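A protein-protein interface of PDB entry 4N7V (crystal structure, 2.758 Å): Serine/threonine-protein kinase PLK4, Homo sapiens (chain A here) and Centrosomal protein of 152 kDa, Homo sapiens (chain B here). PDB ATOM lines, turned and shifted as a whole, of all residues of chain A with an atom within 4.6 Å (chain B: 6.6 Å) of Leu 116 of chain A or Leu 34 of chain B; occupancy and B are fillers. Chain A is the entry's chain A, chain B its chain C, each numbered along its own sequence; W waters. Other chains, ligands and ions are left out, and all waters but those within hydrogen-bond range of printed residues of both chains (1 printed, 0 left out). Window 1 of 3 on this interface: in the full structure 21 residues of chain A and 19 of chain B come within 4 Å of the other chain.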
ATOM      1  N   GLN A  25      31.570  -2.013   2.680  1.00  0.00           N
ATOM      2  CA  GLN A  25      30.547  -1.093   3.164  1.00  0.00           C
ATOM      3  C   GLN A  25      31.121   0.102   3.920  1.00  0.00           C
ATOM      4  O   GLN A  25      31.570  -0.026   5.058  1.00  0.00           O
ATOM      5  CB  GLN A  25      29.544  -1.835   4.050  1.00  0.00           C
ATOM      6  CG  GLN A  25      28.462  -2.578   3.282  1.00  0.00           C
ATOM      7  CD  GLN A  25      27.352  -1.662   2.802  1.00  0.00           C
ATOM      8  OE1 GLN A  25      26.969  -0.717   3.493  1.00  0.00           O
ATOM      9  NE2 GLN A  25      26.827  -1.939   1.613  1.00  0.00           N
ATOM     10  N   ARG A 112      26.950 -10.186  13.080  1.00  0.00           N
ATOM     11  CA  ARG A 112      25.646  -9.758  12.588  1.00  0.00           C
ATOM     12  C   ARG A 112      25.746  -9.393  11.114  1.00  0.00           C
ATOM     13  O   ARG A 112      24.863  -9.721  10.321  1.00  0.00           O
ATOM     14  CB  ARG A 112      25.151  -8.551  13.381  1.00  0.00           C
ATOM     15  CG  ARG A 112      24.755  -8.850  14.815  1.00  0.00           C
ATOM     16  CD  ARG A 112      24.556  -7.556  15.591  1.00  0.00           C
ATOM     17  NE  ARG A 112      24.003  -7.777  16.923  1.00  0.00           N
ATOM     18  CZ  ARG A 112      22.721  -7.615  17.235  1.00  0.00           C
ATOM     19  NH1 ARG A 112      21.855  -7.228  16.307  1.00  0.00           N
ATOM     20  NH2 ARG A 112      22.305  -7.838  18.475  1.00  0.00           N
ATOM     21  N   PHE A 113      26.829  -8.707  10.764  1.00  0.00           N
ATOM     22  CA  PHE A 113      27.095  -8.307   9.386  1.00  0.00           C
ATOM     23  C   PHE A 113      27.120  -9.515   8.464  1.00  0.00           C
ATOM     24  O   PHE A 113      26.514  -9.502   7.395  1.00  0.00           O
ATOM     25  CB  PHE A 113      28.435  -7.579   9.307  1.00  0.00           C
ATOM     26  CG  PHE A 113      28.718  -6.964   7.967  1.00  0.00           C
ATOM     27  CD1 PHE A 113      28.301  -5.673   7.682  1.00  0.00           C
ATOM     28  CD2 PHE A 113      29.423  -7.664   7.000  1.00  0.00           C
ATOM     29  CE1 PHE A 113      28.572  -5.098   6.456  1.00  0.00           C
ATOM     30  CE2 PHE A 113      29.695  -7.094   5.772  1.00  0.00           C
ATOM     31  CZ  PHE A 113      29.268  -5.810   5.500  1.00  0.00           C
ATOM     32  N   VAL A 114      27.831 -10.556   8.883  1.00  0.00           N
ATOM     33  CA  VAL A 114      27.938 -11.775   8.094  1.00  0.00           C
ATOM     34  C   VAL A 114      26.590 -12.482   8.000  1.00  0.00           C
ATOM     35  O   VAL A 114      26.172 -12.895   6.916  1.00  0.00           O
ATOM     36  CB  VAL A 114      29.000 -12.729   8.678  1.00  0.00           C
ATOM     37  CG1 VAL A 114      28.955 -14.072   7.973  1.00  0.00           C
ATOM     38  CG2 VAL A 114      30.383 -12.109   8.566  1.00  0.00           C
ATOM     39  N   GLN A 115      25.911 -12.594   9.139  1.00  0.00           N
ATOM     40  CA  GLN A 115      24.610 -13.255   9.215  1.00  0.00           C
ATOM     41  C   GLN A 115      23.573 -12.544   8.348  1.00  0.00           C
ATOM     42  O   GLN A 115      22.652 -13.167   7.827  1.00  0.00           O
ATOM     43  CB  GLN A 115      24.125 -13.326  10.667  1.00  0.00           C
ATOM     44  CG  GLN A 115      23.705 -14.719  11.113  1.00  0.00           C
ATOM     45  CD  GLN A 115      24.822 -15.731  10.958  1.00  0.00           C
ATOM     46  OE1 GLN A 115      24.698 -16.697  10.204  1.00  0.00           O
ATOM     47  NE2 GLN A 115      25.928 -15.507  11.662  1.00  0.00           N
ATOM     48  N   LEU A 116      23.739 -11.235   8.196  1.00  0.00           N
ATOM     49  CA  LEU A 116      22.869 -10.443   7.336  1.00  0.00           C
ATOM     50  C   LEU A 116      23.155 -10.736   5.868  1.00  0.00           C
ATOM     51  O   LEU A 116      22.236 -10.896   5.063  1.00  0.00           O
ATOM     52  CB  LEU A 116      23.064  -8.953   7.625  1.00  0.00           C
ATOM     53  CG  LEU A 116      21.836  -8.190   8.133  1.00  0.00           C
ATOM     54  CD1 LEU A 116      20.997  -9.050   9.080  1.00  0.00           C
ATOM     55  CD2 LEU A 116      22.262  -6.894   8.809  1.00  0.00           C
ATOM     56  N   VAL A 117      24.438 -10.795   5.528  1.00  0.00           N
ATOM     57  CA  VAL A 117      24.865 -11.067   4.162  1.00  0.00           C
ATOM     58  C   VAL A 117      24.410 -12.453   3.702  1.00  0.00           C
ATOM     59  O   VAL A 117      23.934 -12.617   2.583  1.00  0.00           O
ATOM     60  CB  VAL A 117      26.396 -10.944   4.012  1.00  0.00           C
ATOM     61  CG1 VAL A 117      26.849 -11.474   2.666  1.00  0.00           C
ATOM     62  CG2 VAL A 117      26.836  -9.497   4.198  1.00  0.00           C
ATOM     63  N   ARG A 118      24.541 -13.443   4.578  1.00  0.00           N
ATOM     64  CA  ARG A 118      24.126 -14.806   4.255  1.00  0.00           C
ATOM     65  C   ARG A 118      22.623 -14.900   4.037  1.00  0.00           C
ATOM     66  O   ARG A 118      22.154 -15.743   3.275  1.00  0.00           O
ATOM     67  CB  ARG A 118      24.546 -15.777   5.360  1.00  0.00           C
ATOM     68  CG  ARG A 118      26.046 -15.883   5.567  1.00  0.00           C
ATOM     69  CD  ARG A 118      26.357 -16.755   6.766  1.00  0.00           C
ATOM     70  NE  ARG A 118      25.861 -18.117   6.592  1.00  0.00           N
ATOM     71  CZ  ARG A 118      25.580 -18.942   7.595  1.00  0.00           C
ATOM     72  NH1 ARG A 118      25.733 -18.540   8.849  1.00  0.00           N
ATOM     73  NH2 ARG A 118      25.136 -20.165   7.345  1.00  0.00           N
ATOM     74  N   SER A 119      21.872 -14.033   4.709  1.00  0.00           N
ATOM     75  CA  SER A 119      20.419 -14.019   4.581  1.00  0.00           C
ATOM     76  C   SER A 119      19.975 -13.437   3.240  1.00  0.00           C
ATOM     77  O   SER A 119      18.788 -13.449   2.910  1.00  0.00           O
ATOM     78  CB  SER A 119      19.784 -13.235   5.731  1.00  0.00           C
ATOM     79  OG  SER A 119      20.141 -11.865   5.678  1.00  0.00           O
ATOM     80  N   LYS A 120      20.935 -12.930   2.472  1.00  0.00           N
ATOM     81  CA  LYS A 120      20.671 -12.399   1.138  1.00  0.00           C
ATOM     82  C   LYS A 120      21.632 -13.002   0.124  1.00  0.00           C
ATOM     83  O   LYS A 120      21.903 -12.413  -0.922  1.00  0.00           O
ATOM     84  CB  LYS A 120      20.788 -10.874   1.124  1.00  0.00           C
ATOM     85  CG  LYS A 120      19.763 -10.176   1.990  1.00  0.00           C
ATOM     86  CD  LYS A 120      18.357 -10.513   1.535  1.00  0.00           C
ATOM     87  CE  LYS A 120      17.342 -10.215   2.623  1.00  0.00           C
ATOM     88  NZ  LYS A 120      17.393  -8.787   3.027  1.00  0.00           N
ATOM     89  N   GLU B  29      17.833  -4.686  -0.376  1.00  0.00           N
ATOM     90  CA  GLU B  29      17.392  -5.049   0.966  1.00  0.00           C
ATOM     91  C   GLU B  29      18.602  -5.284   1.869  1.00  0.00           C
ATOM     92  O   GLU B  29      18.559  -5.010   3.068  1.00  0.00           O
ATOM     93  CB  GLU B  29      16.512  -6.302   0.921  1.00  0.00           C
ATOM     94  CG  GLU B  29      15.174  -6.178   1.656  1.00  0.00           C
ATOM     95  CD  GLU B  29      15.271  -6.501   3.140  1.00  0.00           C
ATOM     96  OE1 GLU B  29      14.605  -7.460   3.590  1.00  0.00           O
ATOM     97  OE2 GLU B  29      16.009  -5.797   3.857  1.00  0.00           O
ATOM     98  N   LEU B  30      19.682  -5.788   1.279  1.00  0.00           N
ATOM     99  CA  LEU B  30      20.923  -6.015   2.007  1.00  0.00           C
ATOM    100  C   LEU B  30      21.517  -4.677   2.427  1.00  0.00           C
ATOM    101  O   LEU B  30      21.938  -4.510   3.572  1.00  0.00           O
ATOM    102  CB  LEU B  30      21.923  -6.776   1.137  1.00  0.00           C
ATOM    103  CG  LEU B  30      22.772  -7.878   1.784  1.00  0.00           C
ATOM    104  CD1 LEU B  30      24.047  -8.111   0.981  1.00  0.00           C
ATOM    105  CD2 LEU B  30      23.093  -7.578   3.240  1.00  0.00           C
ATOM    106  N   GLN B  31      21.553  -3.733   1.488  1.00  0.00           N
ATOM    107  CA  GLN B  31      22.078  -2.396   1.743  1.00  0.00           C
ATOM    108  C   GLN B  31      21.337  -1.717   2.887  1.00  0.00           C
ATOM    109  O   GLN B  31      21.951  -1.115   3.763  1.00  0.00           O
ATOM    110  CB  GLN B  31      21.976  -1.531   0.487  1.00  0.00           C
ATOM    111  CG  GLN B  31      22.863  -1.985  -0.653  1.00  0.00           C
ATOM    112  CD  GLN B  31      24.336  -1.845  -0.338  1.00  0.00           C
ATOM    113  OE1 GLN B  31      24.753  -0.902   0.336  1.00  0.00           O
ATOM    114  NE2 GLN B  31      25.135  -2.786  -0.825  1.00  0.00           N
ATOM    115  N   GLN B  32      20.015  -1.818   2.875  1.00  0.00           N
ATOM    116  CA  GLN B  32      19.207  -1.252   3.948  1.00  0.00           C
ATOM    117  C   GLN B  32      19.494  -1.941   5.279  1.00  0.00           C
ATOM    118  O   GLN B  32      19.544  -1.295   6.327  1.00  0.00           O
ATOM    119  CB  GLN B  32      17.720  -1.366   3.615  1.00  0.00           C
ATOM    120  CG  GLN B  32      16.801  -0.859   4.716  1.00  0.00           C
ATOM    121  CD  GLN B  32      17.040   0.602   5.049  1.00  0.00           C
ATOM    122  OE1 GLN B  32      17.258   1.428   4.161  1.00  0.00           O
ATOM    123  NE2 GLN B  32      17.012   0.927   6.336  1.00  0.00           N
ATOM    124  N   LEU B  33      19.683  -3.254   5.225  1.00  0.00           N
ATOM    125  CA  LEU B  33      19.933  -4.055   6.416  1.00  0.00           C
ATOM    126  C   LEU B  33      21.281  -3.727   7.051  1.00  0.00           C
ATOM    127  O   LEU B  33      21.396  -3.632   8.274  1.00  0.00           O
ATOM    128  CB  LEU B  33      19.858  -5.540   6.065  1.00  0.00           C
ATOM    129  CG  LEU B  33      18.741  -6.332   6.745  1.00  0.00           C
ATOM    130  CD1 LEU B  33      17.437  -5.540   6.790  1.00  0.00           C
ATOM    131  CD2 LEU B  33      18.540  -7.664   6.038  1.00  0.00           C
ATOM    132  N   LEU B  34      22.296  -3.546   6.213  1.00  0.00           N
ATOM    133  CA  LEU B  34      23.633  -3.223   6.696  1.00  0.00           C
ATOM    134  C   LEU B  34      23.703  -1.795   7.221  1.00  0.00           C
ATOM    135  O   LEU B  34      24.582  -1.460   8.014  1.00  0.00           O
ATOM    136  CB  LEU B  34      24.670  -3.438   5.594  1.00  0.00           C
ATOM    137  CG  LEU B  34      24.782  -4.868   5.064  1.00  0.00           C
ATOM    138  CD1 LEU B  34      25.863  -4.972   3.998  1.00  0.00           C
ATOM    139  CD2 LEU B  34      25.053  -5.833   6.201  1.00  0.00           C
ATOM    140  N   THR B  35      22.773  -0.958   6.777  1.00  0.00           N
ATOM    141  CA  THR B  35      22.684   0.410   7.271  1.00  0.00           C
ATOM    142  C   THR B  35      22.023   0.423   8.649  1.00  0.00           C
ATOM    143  O   THR B  35      22.404   1.203   9.525  1.00  0.00           O
ATOM    144  CB  THR B  35      21.901   1.310   6.293  1.00  0.00           C
ATOM    145  OG1 THR B  35      22.585   1.355   5.033  1.00  0.00           O
ATOM    146  CG2 THR B  35      21.776   2.725   6.837  1.00  0.00           C
ATOM    147  N   ASP B  36      21.045  -0.458   8.839  1.00  0.00           N
ATOM    148  CA  ASP B  36      20.319  -0.557  10.105  1.00  0.00           C
ATOM    149  C   ASP B  36      21.139  -1.271  11.171  1.00  0.00           C
ATOM    150  O   ASP B  36      20.713  -1.400  12.320  1.00  0.00           O
ATOM    151  CB  ASP B  36      18.993  -1.289   9.906  1.00  0.00           C
ATOM    152  CG  ASP B  36      18.025  -0.512   9.039  1.00  0.00           C
ATOM    153  OD1 ASP B  36      16.815  -0.824   9.068  1.00  0.00           O
ATOM    154  OD2 ASP B  36      18.478   0.415   8.333  1.00  0.00           O
ATOM    155  N   LEU B  37      22.313  -1.743  10.774  1.00  0.00           N
ATOM    156  CA  LEU B  37      23.216  -2.415  11.689  1.00  0.00           C
ATOM    157  C   LEU B  37      23.671  -1.431  12.763  1.00  0.00           C
ATOM    158  O   LEU B  37      24.126  -0.335  12.443  1.00  0.00           O
ATOM    159  CB  LEU B  37      24.420  -2.952  10.918  1.00  0.00           C
ATOM    160  CG  LEU B  37      25.114  -4.183  11.492  1.00  0.00           C
ATOM    161  CD1 LEU B  37      24.107  -5.298  11.722  1.00  0.00           C
ATOM    162  CD2 LEU B  37      26.222  -4.641  10.557  1.00  0.00           C
ATOM    163  N   PRO B  38      23.542  -1.840  14.016  1.00  0.00           N
ATOM    164  CA  PRO B  38      23.903  -0.898  15.052  1.00  0.00           C
ATOM    165  C   PRO B  38      25.341  -0.592  14.742  1.00  0.00           C
ATOM    166  O   PRO B  38      26.198  -1.471  14.654  1.00  0.00           O
ATOM    167  CB  PRO B  38      23.800  -1.729  16.328  1.00  0.00           C
ATOM    168  CG  PRO B  38      24.122  -3.115  15.888  1.00  0.00           C
ATOM    169  CD  PRO B  38      23.580  -3.236  14.491  1.00  0.00           C
ATOM    170  N   HIS B  39      25.586   0.693  14.587  1.00  0.00           N
ATOM    171  CA  HIS B  39      26.931   1.240  14.449  1.00  0.00           C
ATOM    172  C   HIS B  39      27.505   1.715  15.780  1.00  0.00           C
ATOM    173  O   HIS B  39      28.688   2.042  15.871  1.00  0.00           O
ATOM    174  CB  HIS B  39      26.944   2.384  13.433  1.00  0.00           C
ATOM    175  CG  HIS B  39      26.748   1.933  12.019  1.00  0.00           C
ATOM    176  ND1 HIS B  39      25.635   1.234  11.606  1.00  0.00           N
ATOM    177  CD2 HIS B  39      27.527   2.081  10.923  1.00  0.00           C
ATOM    178  CE1 HIS B  39      25.737   0.971  10.316  1.00  0.00           C
ATOM    179  NE2 HIS B  39      26.876   1.475   9.877  1.00  0.00           N
HETATM  180  O   HOH W   1      26.213  -0.110   6.395  1.00  0.00           O
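NE2 of Gln 25 of chain A sits at hydrogen-bond distance from OE1 of Gln 31 of chain B, 2.6 Å away.
The side-chain amino group (NZ) of Lys 120 of chain A lies within salt-bridge range of the side-chain carboxylate (OE1) of Glu 29 of chain B, at 3.1 Å.
OG1 of Thr 35 of chain B is in hydrogen-bond range of O of Gln 31 of chain B, at 2.8 Å.
Among the printed residues, pairs that only touch across the chains: Lys 120 of chain A with Leu 33 of chain B (3.4 Å), Leu 116 of chain A with Leu 33 of chain B (3.4 Å), Phe 113 of chain A with Leu 34 of chain B (3.6 Å), Gln 25 of chain A with Leu 34 of chain B (3.6 Å), Lys 120 of chain A with Leu 30 of chain B (3.7 Å), Phe 113 of chain A with Leu 37 of chain B (3.7 Å), Arg 112 of chain A with Leu 37 of chain B (3.8 Å), Leu 116 of chain A with Leu 37 of chain B (3.8 Å), Leu 116 of chain A with Leu 30 of chain B (3.9 Å) and Leu 116 of chain A with Leu 34 of chain B (3.96 Å).
Of the printed residues of chain B, Gln 25 of chain A touches Gln 31 and Leu 34.
Printed residues of chain B within 4 Å of Phe 113 of chain A: Leu 34 (3.6 Å) and Leu 37 (3.7 Å).
Arg 118 of chain A touches none of the printed residues of chain B.
Of the printed residues of chain A, Leu 30 of chain B touches Leu 116 (3.9 Å) and Lys 120 (3.7 Å).
Gln 32 of chain B touches none of the printed residues of chain A.
Of the printed residues of chain A, Leu 33 of chain B touches Leu 116 and Lys 120.
Printed residues of chain A within 4 Å of Leu 34 of chain B: Gln 25, Phe 113 and Leu 116.
Hydrophobic or aromatic side chains of chain A that line the printed part of chain B: Phe 113 and Leu 116.
Hydrophobic or aromatic side chains of chain B that line the printed part of chain A: Leu 30, Leu 33, Leu 34 and Leu 37.
Among the printed residues, 12 pairs touch across the chains.
Water W1 lies within hydrogen-bond range of the backbone carbonyl oxygen (O) of Leu 34 of chain B and the side-chain amide oxygen (OE1) of Gln 25 of chain A.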
